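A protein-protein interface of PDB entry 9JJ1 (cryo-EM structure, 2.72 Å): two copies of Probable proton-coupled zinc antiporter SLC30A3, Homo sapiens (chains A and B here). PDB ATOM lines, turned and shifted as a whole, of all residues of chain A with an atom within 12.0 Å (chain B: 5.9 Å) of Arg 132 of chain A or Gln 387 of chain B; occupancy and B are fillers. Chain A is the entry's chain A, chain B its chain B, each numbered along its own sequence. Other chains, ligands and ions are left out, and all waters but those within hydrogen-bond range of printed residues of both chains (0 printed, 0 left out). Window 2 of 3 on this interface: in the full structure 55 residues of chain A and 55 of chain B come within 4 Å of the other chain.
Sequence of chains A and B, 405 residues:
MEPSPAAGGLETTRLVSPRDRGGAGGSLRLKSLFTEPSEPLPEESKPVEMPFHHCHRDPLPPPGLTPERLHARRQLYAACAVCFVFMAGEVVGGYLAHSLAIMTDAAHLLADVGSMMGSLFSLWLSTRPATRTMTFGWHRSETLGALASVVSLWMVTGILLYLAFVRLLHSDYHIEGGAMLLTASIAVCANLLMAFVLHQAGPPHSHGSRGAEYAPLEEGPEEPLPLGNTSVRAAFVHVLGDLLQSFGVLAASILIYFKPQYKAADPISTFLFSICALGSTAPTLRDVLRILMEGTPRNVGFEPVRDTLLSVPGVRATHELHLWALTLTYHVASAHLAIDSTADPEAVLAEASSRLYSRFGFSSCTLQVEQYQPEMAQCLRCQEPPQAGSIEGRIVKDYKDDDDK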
ATOM      1  N   ARG A 128       4.955  -9.600 -28.298  1.00  0.00           N
ATOM      2  CA  ARG A 128       6.252 -10.237 -28.173  1.00  0.00           C
ATOM      3  C   ARG A 128       7.098  -9.494 -27.144  1.00  0.00           C
ATOM      4  O   ARG A 128       7.008  -8.269 -27.033  1.00  0.00           O
ATOM      5  CB  ARG A 128       6.966 -10.259 -29.521  1.00  0.00           C
ATOM      6  CG  ARG A 128       6.195 -10.979 -30.605  1.00  0.00           C
ATOM      7  CD  ARG A 128       6.588 -10.479 -31.977  1.00  0.00           C
ATOM      8  NE  ARG A 128       7.896 -10.980 -32.374  1.00  0.00           N
ATOM      9  CZ  ARG A 128       8.364 -10.960 -33.614  1.00  0.00           C
ATOM     10  NH1 ARG A 128       7.653 -10.465 -34.613  1.00  0.00           N
ATOM     11  NH2 ARG A 128       9.575 -11.451 -33.858  1.00  0.00           N
ATOM     12  N   PRO A 129       7.922 -10.203 -26.379  1.00  0.00           N
ATOM     13  CA  PRO A 129       8.784  -9.525 -25.410  1.00  0.00           C
ATOM     14  C   PRO A 129       9.855  -8.705 -26.106  1.00  0.00           C
ATOM     15  O   PRO A 129      10.243  -8.982 -27.243  1.00  0.00           O
ATOM     16  CB  PRO A 129       9.397 -10.680 -24.613  1.00  0.00           C
ATOM     17  CG  PRO A 129       9.353 -11.836 -25.548  1.00  0.00           C
ATOM     18  CD  PRO A 129       8.114 -11.662 -26.371  1.00  0.00           C
ATOM     19  N   ALA A 130      10.321  -7.671 -25.412  1.00  0.00           N
ATOM     20  CA  ALA A 130      11.399  -6.846 -25.936  1.00  0.00           C
ATOM     21  C   ALA A 130      12.665  -7.675 -26.094  1.00  0.00           C
ATOM     22  O   ALA A 130      13.031  -8.446 -25.204  1.00  0.00           O
ATOM     23  CB  ALA A 130      11.652  -5.659 -25.010  1.00  0.00           C
ATOM     24  N   THR A 131      13.329  -7.520 -27.232  1.00  0.00           N
ATOM     25  CA  THR A 131      14.547  -8.252 -27.529  1.00  0.00           C
ATOM     26  C   THR A 131      15.763  -7.367 -27.270  1.00  0.00           C
ATOM     27  O   THR A 131      15.653  -6.227 -26.817  1.00  0.00           O
ATOM     28  CB  THR A 131      14.530  -8.754 -28.974  1.00  0.00           C
ATOM     29  OG1 THR A 131      14.792  -7.662 -29.862  1.00  0.00           O
ATOM     30  CG2 THR A 131      13.178  -9.348 -29.308  1.00  0.00           C
ATOM     31  N   ARG A 132      16.943  -7.910 -27.559  1.00  0.00           N
ATOM     32  CA  ARG A 132      18.177  -7.154 -27.408  1.00  0.00           C
ATOM     33  C   ARG A 132      18.402  -6.163 -28.536  1.00  0.00           C
ATOM     34  O   ARG A 132      19.252  -5.278 -28.400  1.00  0.00           O
ATOM     35  CB  ARG A 132      19.367  -8.107 -27.314  1.00  0.00           C
ATOM     36  CG  ARG A 132      19.390  -8.916 -26.036  1.00  0.00           C
ATOM     37  CD  ARG A 132      20.201 -10.182 -26.200  1.00  0.00           C
ATOM     38  NE  ARG A 132      21.342 -10.215 -25.295  1.00  0.00           N
ATOM     39  CZ  ARG A 132      21.313 -10.725 -24.073  1.00  0.00           C
ATOM     40  NH1 ARG A 132      20.210 -11.257 -23.573  1.00  0.00           N
ATOM     41  NH2 ARG A 132      22.417 -10.701 -23.333  1.00  0.00           N
ATOM     42  N   THR A 133      17.673  -6.289 -29.643  1.00  0.00           N
ATOM     43  CA  THR A 133      17.744  -5.318 -30.724  1.00  0.00           C
ATOM     44  C   THR A 133      16.576  -4.346 -30.723  1.00  0.00           C
ATOM     45  O   THR A 133      16.658  -3.304 -31.380  1.00  0.00           O
ATOM     46  CB  THR A 133      17.799  -6.031 -32.078  1.00  0.00           C
ATOM     47  OG1 THR A 133      16.644  -6.863 -32.228  1.00  0.00           O
ATOM     48  CG2 THR A 133      19.045  -6.889 -32.170  1.00  0.00           C
ATOM     49  N   MET A 134      15.497  -4.662 -30.010  1.00  0.00           N
ATOM     50  CA  MET A 134      14.337  -3.784 -29.865  1.00  0.00           C
ATOM     51  C   MET A 134      14.073  -3.683 -28.368  1.00  0.00           C
ATOM     52  O   MET A 134      13.264  -4.436 -27.821  1.00  0.00           O
ATOM     53  CB  MET A 134      13.133  -4.326 -30.622  1.00  0.00           C
ATOM     54  CG  MET A 134      13.421  -4.669 -32.071  1.00  0.00           C
ATOM     55  SD  MET A 134      13.237  -3.268 -33.182  1.00  0.00           S
ATOM     56  CE  MET A 134      11.850  -2.445 -32.423  1.00  0.00           C
ATOM     57  N   THR A 135      14.759  -2.750 -27.710  1.00  0.00           N
ATOM     58  CA  THR A 135      14.700  -2.674 -26.255  1.00  0.00           C
ATOM     59  C   THR A 135      13.349  -2.164 -25.775  1.00  0.00           C
ATOM     60  O   THR A 135      12.860  -2.584 -24.719  1.00  0.00           O
ATOM     61  CB  THR A 135      15.822  -1.780 -25.735  1.00  0.00           C
ATOM     62  OG1 THR A 135      15.951  -0.638 -26.587  1.00  0.00           O
ATOM     63  CG2 THR A 135      17.133  -2.538 -25.724  1.00  0.00           C
ATOM     64  N   PHE A 136      12.732  -1.256 -26.526  1.00  0.00           N
ATOM     65  CA  PHE A 136      11.461  -0.676 -26.121  1.00  0.00           C
ATOM     66  C   PHE A 136      10.269  -1.568 -26.430  1.00  0.00           C
ATOM     67  O   PHE A 136       9.182  -1.324 -25.896  1.00  0.00           O
ATOM     68  CB  PHE A 136      11.265   0.677 -26.804  1.00  0.00           C
ATOM     69  CG  PHE A 136      11.953   1.810 -26.110  1.00  0.00           C
ATOM     70  CD1 PHE A 136      11.401   2.385 -24.983  1.00  0.00           C
ATOM     71  CD2 PHE A 136      13.152   2.303 -26.586  1.00  0.00           C
ATOM     72  CE1 PHE A 136      12.032   3.429 -24.346  1.00  0.00           C
ATOM     73  CE2 PHE A 136      13.785   3.344 -25.953  1.00  0.00           C
ATOM     74  CZ  PHE A 136      13.224   3.908 -24.832  1.00  0.00           C
ATOM     75  N   GLY A 137      10.438  -2.585 -27.267  1.00  0.00           N
ATOM     76  CA  GLY A 137       9.324  -3.412 -27.675  1.00  0.00           C
ATOM     77  C   GLY A 137       8.974  -3.198 -29.131  1.00  0.00           C
ATOM     78  O   GLY A 137       9.850  -2.883 -29.939  1.00  0.00           O
ATOM     79  N   TRP A 138       7.699  -3.351 -29.480  1.00  0.00           N
ATOM     80  CA  TRP A 138       7.253  -3.201 -30.859  1.00  0.00           C
ATOM     81  C   TRP A 138       6.089  -2.227 -30.961  1.00  0.00           C
ATOM     82  O   TRP A 138       5.257  -2.338 -31.864  1.00  0.00           O
ATOM     83  CB  TRP A 138       6.872  -4.553 -31.457  1.00  0.00           C
ATOM     84  CG  TRP A 138       7.955  -5.574 -31.359  1.00  0.00           C
ATOM     85  CD1 TRP A 138       8.266  -6.336 -30.275  1.00  0.00           C
ATOM     86  CD2 TRP A 138       8.874  -5.945 -32.388  1.00  0.00           C
ATOM     87  NE1 TRP A 138       9.324  -7.160 -30.563  1.00  0.00           N
ATOM     88  CE2 TRP A 138       9.715  -6.939 -31.857  1.00  0.00           C
ATOM     89  CE3 TRP A 138       9.067  -5.535 -33.709  1.00  0.00           C
ATOM     90  CZ2 TRP A 138      10.732  -7.527 -32.597  1.00  0.00           C
ATOM     91  CZ3 TRP A 138      10.076  -6.120 -34.441  1.00  0.00           C
ATOM     92  CH2 TRP A 138      10.896  -7.106 -33.885  1.00  0.00           C
ATOM     93  N   THR B 296      17.841  -0.873 -31.509  1.00  0.00           N
ATOM     94  CA  THR B 296      19.231  -0.644 -31.154  1.00  0.00           C
ATOM     95  C   THR B 296      20.013  -0.190 -32.383  1.00  0.00           C
ATOM     96  O   THR B 296      19.781  -0.698 -33.487  1.00  0.00           O
ATOM     97  CB  THR B 296      19.844  -1.923 -30.581  1.00  0.00           C
ATOM     98  OG1 THR B 296      19.010  -2.417 -29.528  1.00  0.00           O
ATOM     99  CG2 THR B 296      21.228  -1.666 -30.028  1.00  0.00           C
ATOM    100  N   PHE B 302      24.039  -4.593 -27.651  1.00  0.00           N
ATOM    101  CA  PHE B 302      23.434  -4.640 -26.324  1.00  0.00           C
ATOM    102  C   PHE B 302      24.393  -5.237 -25.303  1.00  0.00           C
ATOM    103  O   PHE B 302      24.599  -4.675 -24.221  1.00  0.00           O
ATOM    104  CB  PHE B 302      22.137  -5.446 -26.384  1.00  0.00           C
ATOM    105  CG  PHE B 302      21.346  -5.431 -25.111  1.00  0.00           C
ATOM    106  CD1 PHE B 302      21.585  -6.367 -24.121  1.00  0.00           C
ATOM    107  CD2 PHE B 302      20.350  -4.497 -24.912  1.00  0.00           C
ATOM    108  CE1 PHE B 302      20.857  -6.359 -22.956  1.00  0.00           C
ATOM    109  CE2 PHE B 302      19.619  -4.488 -23.748  1.00  0.00           C
ATOM    110  CZ  PHE B 302      19.872  -5.419 -22.770  1.00  0.00           C
ATOM    111  N   GLU B 303      24.980  -6.387 -25.627  1.00  0.00           N
ATOM    112  CA  GLU B 303      25.876  -7.061 -24.690  1.00  0.00           C
ATOM    113  C   GLU B 303      27.128  -6.255 -24.366  1.00  0.00           C
ATOM    114  O   GLU B 303      27.516  -6.220 -23.186  1.00  0.00           O
ATOM    115  CB  GLU B 303      26.230  -8.449 -25.227  1.00  0.00           C
ATOM    116  CG  GLU B 303      25.104  -9.450 -25.111  1.00  0.00           C
ATOM    117  CD  GLU B 303      24.247  -9.494 -26.357  1.00  0.00           C
ATOM    118  OE1 GLU B 303      24.426  -8.621 -27.233  1.00  0.00           O
ATOM    119  OE2 GLU B 303      23.398 -10.402 -26.464  1.00  0.00           O
ATOM    120  N   ARG B 306      26.006  -3.572 -21.908  1.00  0.00           N
ATOM    121  CA  ARG B 306      25.646  -4.142 -20.614  1.00  0.00           C
ATOM    122  C   ARG B 306      26.883  -4.569 -19.837  1.00  0.00           C
ATOM    123  O   ARG B 306      26.958  -4.371 -18.620  1.00  0.00           O
ATOM    124  CB  ARG B 306      24.696  -5.322 -20.800  1.00  0.00           C
ATOM    125  CG  ARG B 306      24.133  -5.857 -19.499  1.00  0.00           C
ATOM    126  CD  ARG B 306      23.354  -7.140 -19.710  1.00  0.00           C
ATOM    127  NE  ARG B 306      24.005  -8.023 -20.671  1.00  0.00           N
ATOM    128  CZ  ARG B 306      25.030  -8.813 -20.387  1.00  0.00           C
ATOM    129  NH1 ARG B 306      25.555  -8.856 -19.174  1.00  0.00           N
ATOM    130  NH2 ARG B 306      25.545  -9.579 -21.345  1.00  0.00           N
ATOM    131  N   GLU B 384      16.849  -8.819 -17.958  1.00  0.00           N
ATOM    132  CA  GLU B 384      17.246  -8.413 -19.293  1.00  0.00           C
ATOM    133  C   GLU B 384      16.647  -9.351 -20.341  1.00  0.00           C
ATOM    134  O   GLU B 384      16.299 -10.495 -20.040  1.00  0.00           O
ATOM    135  CB  GLU B 384      18.768  -8.391 -19.408  1.00  0.00           C
ATOM    136  CG  GLU B 384      19.450  -7.499 -18.381  1.00  0.00           C
ATOM    137  CD  GLU B 384      19.545  -6.052 -18.826  1.00  0.00           C
ATOM    138  OE1 GLU B 384      18.502  -5.460 -19.176  1.00  0.00           O
ATOM    139  OE2 GLU B 384      20.665  -5.504 -18.823  1.00  0.00           O
ATOM    140  N   PRO B 385      16.500  -8.874 -21.576  1.00  0.00           N
ATOM    141  CA  PRO B 385      15.971  -9.736 -22.629  1.00  0.00           C
ATOM    142  C   PRO B 385      16.868 -10.938 -22.841  1.00  0.00           C
ATOM    143  O   PRO B 385      18.095 -10.863 -22.647  1.00  0.00           O
ATOM    144  CB  PRO B 385      15.955  -8.823 -23.865  1.00  0.00           C
ATOM    145  CG  PRO B 385      16.489  -7.503 -23.440  1.00  0.00           C
ATOM    146  CD  PRO B 385      16.522  -7.456 -21.962  1.00  0.00           C
ATOM    147  N   PRO B 386      16.298 -12.073 -23.238  1.00  0.00           N
ATOM    148  CA  PRO B 386      17.107 -13.281 -23.423  1.00  0.00           C
ATOM    149  C   PRO B 386      18.005 -13.171 -24.645  1.00  0.00           C
ATOM    150  O   PRO B 386      17.769 -12.382 -25.562  1.00  0.00           O
ATOM    151  CB  PRO B 386      16.069 -14.397 -23.600  1.00  0.00           C
ATOM    152  CG  PRO B 386      14.717 -13.737 -23.558  1.00  0.00           C
ATOM    153  CD  PRO B 386      14.906 -12.263 -23.671  1.00  0.00           C
ATOM    154  N   GLN B 387      19.058 -13.985 -24.636  1.00  0.00           N
ATOM    155  CA  GLN B 387      20.016 -13.992 -25.733  1.00  0.00           C
ATOM    156  C   GLN B 387      19.337 -14.388 -27.039  1.00  0.00           C
ATOM    157  O   GLN B 387      18.452 -15.247 -27.064  1.00  0.00           O
ATOM    158  CB  GLN B 387      21.163 -14.955 -25.425  1.00  0.00           C
ATOM    159  CG  GLN B 387      22.440 -14.673 -26.199  1.00  0.00           C
ATOM    160  CD  GLN B 387      23.502 -14.009 -25.347  1.00  0.00           C
ATOM    161  OE1 GLN B 387      23.208 -13.116 -24.552  1.00  0.00           O
ATOM    162  NE2 GLN B 387      24.746 -14.443 -25.507  1.00  0.00           N
ATOM    163  N   ALA B 388      19.756 -13.751 -28.126  1.00  0.00           N
ATOM    164  CA  ALA B 388      19.200 -14.037 -29.442  1.00  0.00           C
ATOM    165  C   ALA B 388      19.710 -15.373 -29.969  1.00  0.00           C
ATOM    166  O   ALA B 388      20.689 -15.918 -29.458  1.00  0.00           O
ATOM    167  CB  ALA B 388      19.537 -12.920 -30.414  1.00  0.00           C
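NH2 of Arg 132 of chain A sits at hydrogen-bond distance from OE1 of Gln 387 of chain B, 2.8 Å away. O of Arg 132 of chain A is in hydrogen-bond range of OG1 of Thr 296 of chain B, at 3.1 Å. O of Pro 385 of chain B sits close to NH1 of Arg 132 of chain A (2.3 Å). NH1 of Arg 132 of chain A sits close to O of Pro 386 of chain B, 3.3 Å away. The backbone carbonyl oxygen (O) of Thr 133 of chain A lies within hydrogen-bond range of the backbone NH (N) of Thr 296 of chain B (2.7 Å). The guanidinium group (NH2) of Arg 132 of chain A lies within salt-bridge range of the side-chain carboxylate (OE2) of Glu 303 of chain B, 3.3 Å away.
Of the printed residues of chain B, Thr 133 of chain A touches Thr 296. Of chain A, only Arg 132 (3.1 Å) and Thr 133 (2.7 Å) come within 4 Å of Thr 296 of chain B. Glu 303 of chain B touches one residue of chain A. Printed residues of chain A within 4 Å of Arg 306 of chain B: Arg 132 (3.9 Å). Of chain A, only Ala 130, Thr 131 and Arg 132 come within 4 Å of Pro 385 of chain B. Gln 387 of chain B touches just one residue of chain A: Arg 132 (2.8 Å). The nearest residue of chain B that does not touch Arg 132 of chain A is Ala 388 of chain B (4.1 Å). The nearest residue of chain A that does not touch Gln 387 of chain B is Thr 131 of chain A (7.7 Å). The nearest printed residue of chain B that does not touch Ala 130 of chain A is Pro 386 of chain B (4.5 Å).
Pro 385 of chain B touches Ala 130 of chain A (CB to O, 3.2 Å). Thr 131 of chain A touches Pro 385 of chain B (O to CG, 3.7 Å). Phe 302 of chain B touches Arg 132 of chain A (CB to O, 3.5 Å). NH2 of Arg 132 of chain A touches NH2 of Arg 306 of chain B (3.9 Å). Thr 135 of chain A touches Phe 302 of chain B.
No position is printed for both chains. Of the 11 pairs that touch across the chains among the printed residues, none has its exchanged pair printed and touching as well.
OG1 of Thr 131 of chain A is in hydrogen-bond range of OG1 of Thr 133 of chain A, 3.1 Å away. OE2 of Glu 303 of chain B lies close to OE1 of Gln 387 of chain B (3.3 Å). The backbone NH of Met 134 of chain A lies within hydrogen-bond range of the side-chain hydroxyl of Thr 131 of chain A (3.1 Å).
Printed residues of chain B that touch a printed residue of chain A: Thr 296, Phe 302, Glu 303, Arg 306, Pro 385, Pro 386 and Gln 387. Hydrophobic or aromatic side chains of chain B within 4 Å of the printed part of chain A: Phe 302 and Pro 385.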
